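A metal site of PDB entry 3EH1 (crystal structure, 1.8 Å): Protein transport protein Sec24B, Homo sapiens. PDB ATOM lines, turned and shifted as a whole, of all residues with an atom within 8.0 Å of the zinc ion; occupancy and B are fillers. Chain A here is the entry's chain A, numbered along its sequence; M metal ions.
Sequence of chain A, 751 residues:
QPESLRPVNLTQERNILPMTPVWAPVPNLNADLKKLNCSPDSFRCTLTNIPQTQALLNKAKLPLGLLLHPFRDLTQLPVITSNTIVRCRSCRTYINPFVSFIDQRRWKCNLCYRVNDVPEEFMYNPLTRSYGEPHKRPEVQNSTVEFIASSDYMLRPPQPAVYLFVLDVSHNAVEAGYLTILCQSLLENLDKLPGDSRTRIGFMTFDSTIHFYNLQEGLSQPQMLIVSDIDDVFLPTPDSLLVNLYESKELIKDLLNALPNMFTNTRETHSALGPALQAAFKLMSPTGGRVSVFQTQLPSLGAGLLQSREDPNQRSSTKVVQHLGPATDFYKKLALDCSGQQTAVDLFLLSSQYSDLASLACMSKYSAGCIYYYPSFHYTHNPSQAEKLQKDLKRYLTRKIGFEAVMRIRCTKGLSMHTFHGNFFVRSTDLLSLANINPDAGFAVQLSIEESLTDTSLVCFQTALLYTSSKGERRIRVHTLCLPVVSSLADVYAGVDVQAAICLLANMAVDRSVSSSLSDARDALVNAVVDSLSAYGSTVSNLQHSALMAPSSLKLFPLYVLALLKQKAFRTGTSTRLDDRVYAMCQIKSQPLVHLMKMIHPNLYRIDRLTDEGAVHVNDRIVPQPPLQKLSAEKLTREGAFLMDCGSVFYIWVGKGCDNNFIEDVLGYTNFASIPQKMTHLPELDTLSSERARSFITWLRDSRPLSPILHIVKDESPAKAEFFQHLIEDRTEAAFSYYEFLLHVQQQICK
The guanidinium group of Arg 114 is in hydrogen-bond range of the backbone carbonyl oxygen of Cys 112 (2.9 Å). N of Cys 88 is in hydrogen-bond range of O of Thr 93, at 2.8 Å. The side-chain sulfur (SG) of Cys 88 lies close to the backbone NH (N) of Ser 90 (3.4 Å). The side-chain sulfur (SG) of Cys 88 sits close to the side-chain amide nitrogen (ND2) of Asn 116 (3.5 Å). The side-chain sulfur (SG) of Cys 91 sits close to the side-chain hydroxyl (OG1) of Thr 93 (3.0 Å). O of Cys 91 lies within hydrogen-bond range of NE of Arg 410, 2.8 Å away. The side-chain sulfur (SG) of Cys 109 lies close to the backbone NH (N) of Leu 111, at 3.4 Å. O of Arg 114 sits at hydrogen-bond distance from N of Cys 109 (2.9 Å).
The zinc ion is bound by SG of Cys 112, SG of Cys 88, SG of Cys 91 and SG of Cys 109. The zinc ion has four donor atoms within binding distance.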
ATOM      1  N   ARG A  87      10.875  16.204   1.875  1.00  0.00           N
ATOM      2  CA  ARG A  87      10.543  17.305   2.774  1.00  0.00           C
ATOM      3  C   ARG A  87      10.758  18.666   2.096  1.00  0.00           C
ATOM      4  O   ARG A  87      11.593  18.793   1.202  1.00  0.00           O
ATOM      5  CB  ARG A  87      11.420  17.213   4.021  1.00  0.00           C
ATOM      6  CG  ARG A  87      11.411  15.842   4.677  1.00  0.00           C
ATOM      7  CD  ARG A  87      12.398  15.773   5.827  1.00  0.00           C
ATOM      8  NE  ARG A  87      12.053  16.710   6.885  1.00  0.00           N
ATOM      9  CZ  ARG A  87      12.751  16.869   7.997  1.00  0.00           C
ATOM     10  NH1 ARG A  87      13.847  16.143   8.195  1.00  0.00           N
ATOM     11  NH2 ARG A  87      12.359  17.738   8.913  1.00  0.00           N
ATOM     12  N   CYS A  88      10.018  19.671   2.543  1.00  0.00           N
ATOM     13  CA  CYS A  88      10.130  21.020   1.989  1.00  0.00           C
ATOM     14  C   CYS A  88      11.531  21.598   2.189  1.00  0.00           C
ATOM     15  O   CYS A  88      12.106  21.473   3.271  1.00  0.00           O
ATOM     16  CB  CYS A  88       9.106  21.950   2.629  1.00  0.00           C
ATOM     17  SG  CYS A  88       9.234  23.664   2.058  1.00  0.00           S
ATOM     18  N   ARG A  89      12.053  22.250   1.156  1.00  0.00           N
ATOM     19  CA  ARG A  89      13.382  22.839   1.182  1.00  0.00           C
ATOM     20  C   ARG A  89      13.516  24.051   2.107  1.00  0.00           C
ATOM     21  O   ARG A  89      14.616  24.383   2.539  1.00  0.00           O
ATOM     22  CB  ARG A  89      13.788  23.267  -0.234  1.00  0.00           C
ATOM     23  CG  ARG A  89      12.946  24.419  -0.788  1.00  0.00           C
ATOM     24  CD  ARG A  89      13.251  24.693  -2.250  1.00  0.00           C
ATOM     25  NE  ARG A  89      12.312  25.645  -2.841  1.00  0.00           N
ATOM     26  CZ  ARG A  89      12.392  26.971  -2.749  1.00  0.00           C
ATOM     27  NH1 ARG A  89      13.376  27.546  -2.063  1.00  0.00           N
ATOM     28  NH2 ARG A  89      11.465  27.721  -3.335  1.00  0.00           N
ATOM     29  N   SER A  90      12.406  24.708   2.399  1.00  0.00           N
ATOM     30  CA  SER A  90      12.436  25.894   3.244  1.00  0.00           C
ATOM     31  C   SER A  90      11.997  25.731   4.695  1.00  0.00           C
ATOM     32  O   SER A  90      12.552  26.383   5.574  1.00  0.00           O
ATOM     33  CB  SER A  90      11.607  27.017   2.601  1.00  0.00           C
ATOM     34  OG  SER A  90      12.270  27.556   1.473  1.00  0.00           O
ATOM     35  N   CYS A  91      11.013  24.873   4.950  1.00  0.00           N
ATOM     36  CA  CYS A  91      10.554  24.674   6.328  1.00  0.00           C
ATOM     37  C   CYS A  91      10.696  23.234   6.817  1.00  0.00           C
ATOM     38  O   CYS A  91      10.412  22.939   7.984  1.00  0.00           O
ATOM     39  CB  CYS A  91       9.097  25.122   6.465  1.00  0.00           C
ATOM     40  SG  CYS A  91       7.885  24.006   5.706  1.00  0.00           S
ATOM     41  N   ARG A  92      11.131  22.350   5.929  1.00  0.00           N
ATOM     42  CA  ARG A  92      11.359  20.938   6.249  1.00  0.00           C
ATOM     43  C   ARG A  92      10.096  20.119   6.548  1.00  0.00           C
ATOM     44  O   ARG A  92      10.184  19.039   7.129  1.00  0.00           O
ATOM     45  CB  ARG A  92      12.343  20.803   7.411  1.00  0.00           C
ATOM     46  CG  ARG A  92      13.657  21.549   7.211  1.00  0.00           C
ATOM     47  CD  ARG A  92      14.320  21.161   5.895  1.00  0.00           C
ATOM     48  NE  ARG A  92      14.632  19.731   5.824  1.00  0.00           N
ATOM     49  CZ  ARG A  92      15.110  19.131   4.741  1.00  0.00           C
ATOM     50  NH1 ARG A  92      15.327  19.822   3.630  1.00  0.00           N
ATOM     51  NH2 ARG A  92      15.347  17.821   4.765  1.00  0.00           N
ATOM     52  N   THR A  93       8.941  20.641   6.150  1.00  0.00           N
ATOM     53  CA  THR A  93       7.684  19.929   6.354  1.00  0.00           C
ATOM     54  C   THR A  93       7.723  18.655   5.515  1.00  0.00           C
ATOM     55  O   THR A  93       8.230  18.661   4.393  1.00  0.00           O
ATOM     56  CB  THR A  93       6.473  20.800   5.914  1.00  0.00           C
ATOM     57  OG1 THR A  93       6.197  21.786   6.911  1.00  0.00           O
ATOM     58  CG2 THR A  93       5.236  19.940   5.684  1.00  0.00           C
ATOM     59  N   TYR A  94       7.202  17.556   6.061  1.00  0.00           N
ATOM     60  CA  TYR A  94       7.170  16.289   5.337  1.00  0.00           C
ATOM     61  C   TYR A  94       6.029  16.327   4.324  1.00  0.00           C
ATOM     62  O   TYR A  94       4.941  16.806   4.642  1.00  0.00           O
ATOM     63  CB  TYR A  94       6.937  15.131   6.327  1.00  0.00           C
ATOM     64  CG  TYR A  94       8.088  14.929   7.283  1.00  0.00           C
ATOM     65  CD1 TYR A  94       9.100  14.009   6.989  1.00  0.00           C
ATOM     66  CD2 TYR A  94       8.195  15.678   8.442  1.00  0.00           C
ATOM     67  CE1 TYR A  94      10.198  13.855   7.845  1.00  0.00           C
ATOM     68  CE2 TYR A  94       9.290  15.536   9.304  1.00  0.00           C
ATOM     69  CZ  TYR A  94      10.285  14.621   8.995  1.00  0.00           C
ATOM     70  OH  TYR A  94      11.380  14.494   9.819  1.00  0.00           O
ATOM     71  N   TRP A 107       5.819  20.072  -6.175  1.00  0.00           N
ATOM     72  CA  TRP A 107       4.761  20.204  -5.179  1.00  0.00           C
ATOM     73  C   TRP A 107       4.956  21.494  -4.378  1.00  0.00           C
ATOM     74  O   TRP A 107       6.085  21.905  -4.109  1.00  0.00           O
ATOM     75  CB  TRP A 107       4.750  19.004  -4.220  1.00  0.00           C
ATOM     76  CG  TRP A 107       6.020  18.791  -3.427  1.00  0.00           C
ATOM     77  CD1 TRP A 107       7.199  18.276  -3.892  1.00  0.00           C
ATOM     78  CD2 TRP A 107       6.215  19.061  -2.037  1.00  0.00           C
ATOM     79  NE1 TRP A 107       8.114  18.205  -2.876  1.00  0.00           N
ATOM     80  CE2 TRP A 107       7.545  18.677  -1.724  1.00  0.00           C
ATOM     81  CE3 TRP A 107       5.405  19.586  -1.019  1.00  0.00           C
ATOM     82  CZ2 TRP A 107       8.084  18.807  -0.437  1.00  0.00           C
ATOM     83  CZ3 TRP A 107       5.945  19.716   0.268  1.00  0.00           C
ATOM     84  CH2 TRP A 107       7.273  19.322   0.542  1.00  0.00           C
ATOM     85  N   LYS A 108       3.849  22.132  -4.039  1.00  0.00           N
ATOM     86  CA  LYS A 108       3.907  23.358  -3.250  1.00  0.00           C
ATOM     87  C   LYS A 108       3.630  23.006  -1.802  1.00  0.00           C
ATOM     88  O   LYS A 108       2.629  22.365  -1.482  1.00  0.00           O
ATOM     89  CB  LYS A 108       2.886  24.380  -3.736  1.00  0.00           C
ATOM     90  CG  LYS A 108       2.851  25.645  -2.880  1.00  0.00           C
ATOM     91  CD  LYS A 108       1.855  26.672  -3.393  1.00  0.00           C
ATOM     92  CE  LYS A 108       2.291  27.267  -4.727  1.00  0.00           C
ATOM     93  NZ  LYS A 108       1.411  28.405  -5.104  1.00  0.00           N
ATOM     94  N   CYS A 109       4.526  23.442  -0.914  1.00  0.00           N
ATOM     95  CA  CYS A 109       4.382  23.185   0.507  1.00  0.00           C
ATOM     96  C   CYS A 109       3.131  23.878   1.039  1.00  0.00           C
ATOM     97  O   CYS A 109       2.884  25.045   0.731  1.00  0.00           O
ATOM     98  CB  CYS A 109       5.615  23.687   1.265  1.00  0.00           C
ATOM     99  SG  CYS A 109       5.546  23.331   3.021  1.00  0.00           S
ATOM    100  N   ASN A 110       2.342  23.147   1.827  1.00  0.00           N
ATOM    101  CA  ASN A 110       1.117  23.699   2.381  1.00  0.00           C
ATOM    102  C   ASN A 110       1.336  24.468   3.686  1.00  0.00           C
ATOM    103  O   ASN A 110       0.384  24.980   4.280  1.00  0.00           O
ATOM    104  CB  ASN A 110       0.079  22.584   2.570  1.00  0.00           C
ATOM    105  CG  ASN A 110       0.609  21.404   3.383  1.00  0.00           C
ATOM    106  OD1 ASN A 110       1.695  20.893   3.117  1.00  0.00           O
ATOM    107  ND2 ASN A 110      -0.175  20.956   4.357  1.00  0.00           N
ATOM    108  N   LEU A 111       2.591  24.562   4.126  1.00  0.00           N
ATOM    109  CA  LEU A 111       2.895  25.288   5.351  1.00  0.00           C
ATOM    110  C   LEU A 111       3.624  26.617   5.099  1.00  0.00           C
ATOM    111  O   LEU A 111       3.349  27.593   5.777  1.00  0.00           O
ATOM    112  CB  LEU A 111       3.703  24.405   6.314  1.00  0.00           C
ATOM    113  CG  LEU A 111       2.837  23.552   7.265  1.00  0.00           C
ATOM    114  CD1 LEU A 111       2.116  22.463   6.470  1.00  0.00           C
ATOM    115  CD2 LEU A 111       3.703  22.931   8.344  1.00  0.00           C
ATOM    116  N   CYS A 112       4.538  26.643   4.120  1.00  0.00           N
ATOM    117  CA  CYS A 112       5.264  27.889   3.824  1.00  0.00           C
ATOM    118  C   CYS A 112       5.070  28.318   2.370  1.00  0.00           C
ATOM    119  O   CYS A 112       5.552  29.386   1.945  1.00  0.00           O
ATOM    120  CB  CYS A 112       6.763  27.738   4.117  1.00  0.00           C
ATOM    121  SG  CYS A 112       7.702  26.804   2.891  1.00  0.00           S
ATOM    122  N   TYR A 113       4.361  27.488   1.607  1.00  0.00           N
ATOM    123  CA  TYR A 113       4.033  27.758   0.217  1.00  0.00           C
ATOM    124  C   TYR A 113       5.169  27.767  -0.791  1.00  0.00           C
ATOM    125  O   TYR A 113       4.995  28.206  -1.931  1.00  0.00           O
ATOM    126  CB  TYR A 113       3.244  29.069   0.132  1.00  0.00           C
ATOM    127  CG  TYR A 113       2.133  29.165   1.156  1.00  0.00           C
ATOM    128  CD1 TYR A 113       1.134  28.183   1.220  1.00  0.00           C
ATOM    129  CD2 TYR A 113       2.077  30.224   2.057  1.00  0.00           C
ATOM    130  CE1 TYR A 113       0.109  28.260   2.167  1.00  0.00           C
ATOM    131  CE2 TYR A 113       1.057  30.309   3.007  1.00  0.00           C
ATOM    132  CZ  TYR A 113       0.086  29.327   3.052  1.00  0.00           C
ATOM    133  OH  TYR A 113      -0.927  29.430   3.974  1.00  0.00           O
ATOM    134  N   ARG A 114       6.347  27.293  -0.396  1.00  0.00           N
ATOM    135  CA  ARG A 114       7.471  27.240  -1.319  1.00  0.00           C
ATOM    136  C   ARG A 114       7.330  26.033  -2.240  1.00  0.00           C
ATOM    137  O   ARG A 114       6.861  24.968  -1.816  1.00  0.00           O
ATOM    138  CB  ARG A 114       8.794  27.171  -0.566  1.00  0.00           C
ATOM    139  CG  ARG A 114       9.460  28.531  -0.332  1.00  0.00           C
ATOM    140  CD  ARG A 114       8.565  29.468   0.455  1.00  0.00           C
ATOM    141  NE  ARG A 114       9.221  30.752   0.743  1.00  0.00           N
ATOM    142  CZ  ARG A 114       8.672  31.722   1.473  1.00  0.00           C
ATOM    143  NH1 ARG A 114       7.459  31.551   1.994  1.00  0.00           N
ATOM    144  NH2 ARG A 114       9.332  32.855   1.679  1.00  0.00           N
ATOM    145  N   VAL A 115       7.722  26.194  -3.494  1.00  0.00           N
ATOM    146  CA  VAL A 115       7.641  25.120  -4.475  1.00  0.00           C
ATOM    147  C   VAL A 115       8.875  24.231  -4.375  1.00  0.00           C
ATOM    148  O   VAL A 115      10.007  24.715  -4.242  1.00  0.00           O
ATOM    149  CB  VAL A 115       7.532  25.701  -5.913  1.00  0.00           C
ATOM    150  CG1 VAL A 115       7.478  24.570  -6.931  1.00  0.00           C
ATOM    151  CG2 VAL A 115       6.277  26.557  -6.024  1.00  0.00           C
ATOM    152  N   ASN A 116       8.649  22.916  -4.426  1.00  0.00           N
ATOM    153  CA  ASN A 116       9.712  21.926  -4.317  1.00  0.00           C
ATOM    154  C   ASN A 116       9.660  20.951  -5.483  1.00  0.00           C
ATOM    155  O   ASN A 116       8.588  20.690  -6.024  1.00  0.00           O
ATOM    156  CB  ASN A 116       9.571  21.136  -3.011  1.00  0.00           C
ATOM    157  CG  ASN A 116       9.837  21.971  -1.799  1.00  0.00           C
ATOM    158  OD1 ASN A 116      10.968  22.046  -1.316  1.00  0.00           O
ATOM    159  ND2 ASN A 116       8.794  22.625  -1.281  1.00  0.00           N
ATOM    160  N   ARG A 410       5.314  21.388  13.313  1.00  0.00           N
ATOM    161  CA  ARG A 410       5.335  22.469  12.345  1.00  0.00           C
ATOM    162  C   ARG A 410       3.910  22.944  12.070  1.00  0.00           C
ATOM    163  O   ARG A 410       2.963  22.199  12.261  1.00  0.00           O
ATOM    164  CB  ARG A 410       5.991  22.003  11.047  1.00  0.00           C
ATOM    165  CG  ARG A 410       7.471  21.652  11.190  1.00  0.00           C
ATOM    166  CD  ARG A 410       8.122  21.302   9.862  1.00  0.00           C
ATOM    167  NE  ARG A 410       9.571  21.163   9.976  1.00  0.00           N
ATOM    168  CZ  ARG A 410      10.193  20.110  10.510  1.00  0.00           C
ATOM    169  NH1 ARG A 410       9.498  19.082  10.986  1.00  0.00           N
ATOM    170  NH2 ARG A 410      11.522  20.103  10.597  1.00  0.00           N
ATOM    171  N   CYS A 411       3.767  24.196  11.642  1.00  0.00           N
ATOM    172  CA  CYS A 411       2.448  24.735  11.340  1.00  0.00           C
ATOM    173  C   CYS A 411       2.548  25.780  10.252  1.00  0.00           C
ATOM    174  O   CYS A 411       3.599  26.416  10.058  1.00  0.00           O
ATOM    175  CB  CYS A 411       1.818  25.355  12.587  1.00  0.00           C
ATOM    176  SG  CYS A 411       2.774  26.690  13.307  1.00  0.00           S
HETATM  177 ZN    ZN M   1       7.546  24.561   3.426  1.00  0.00          ZN
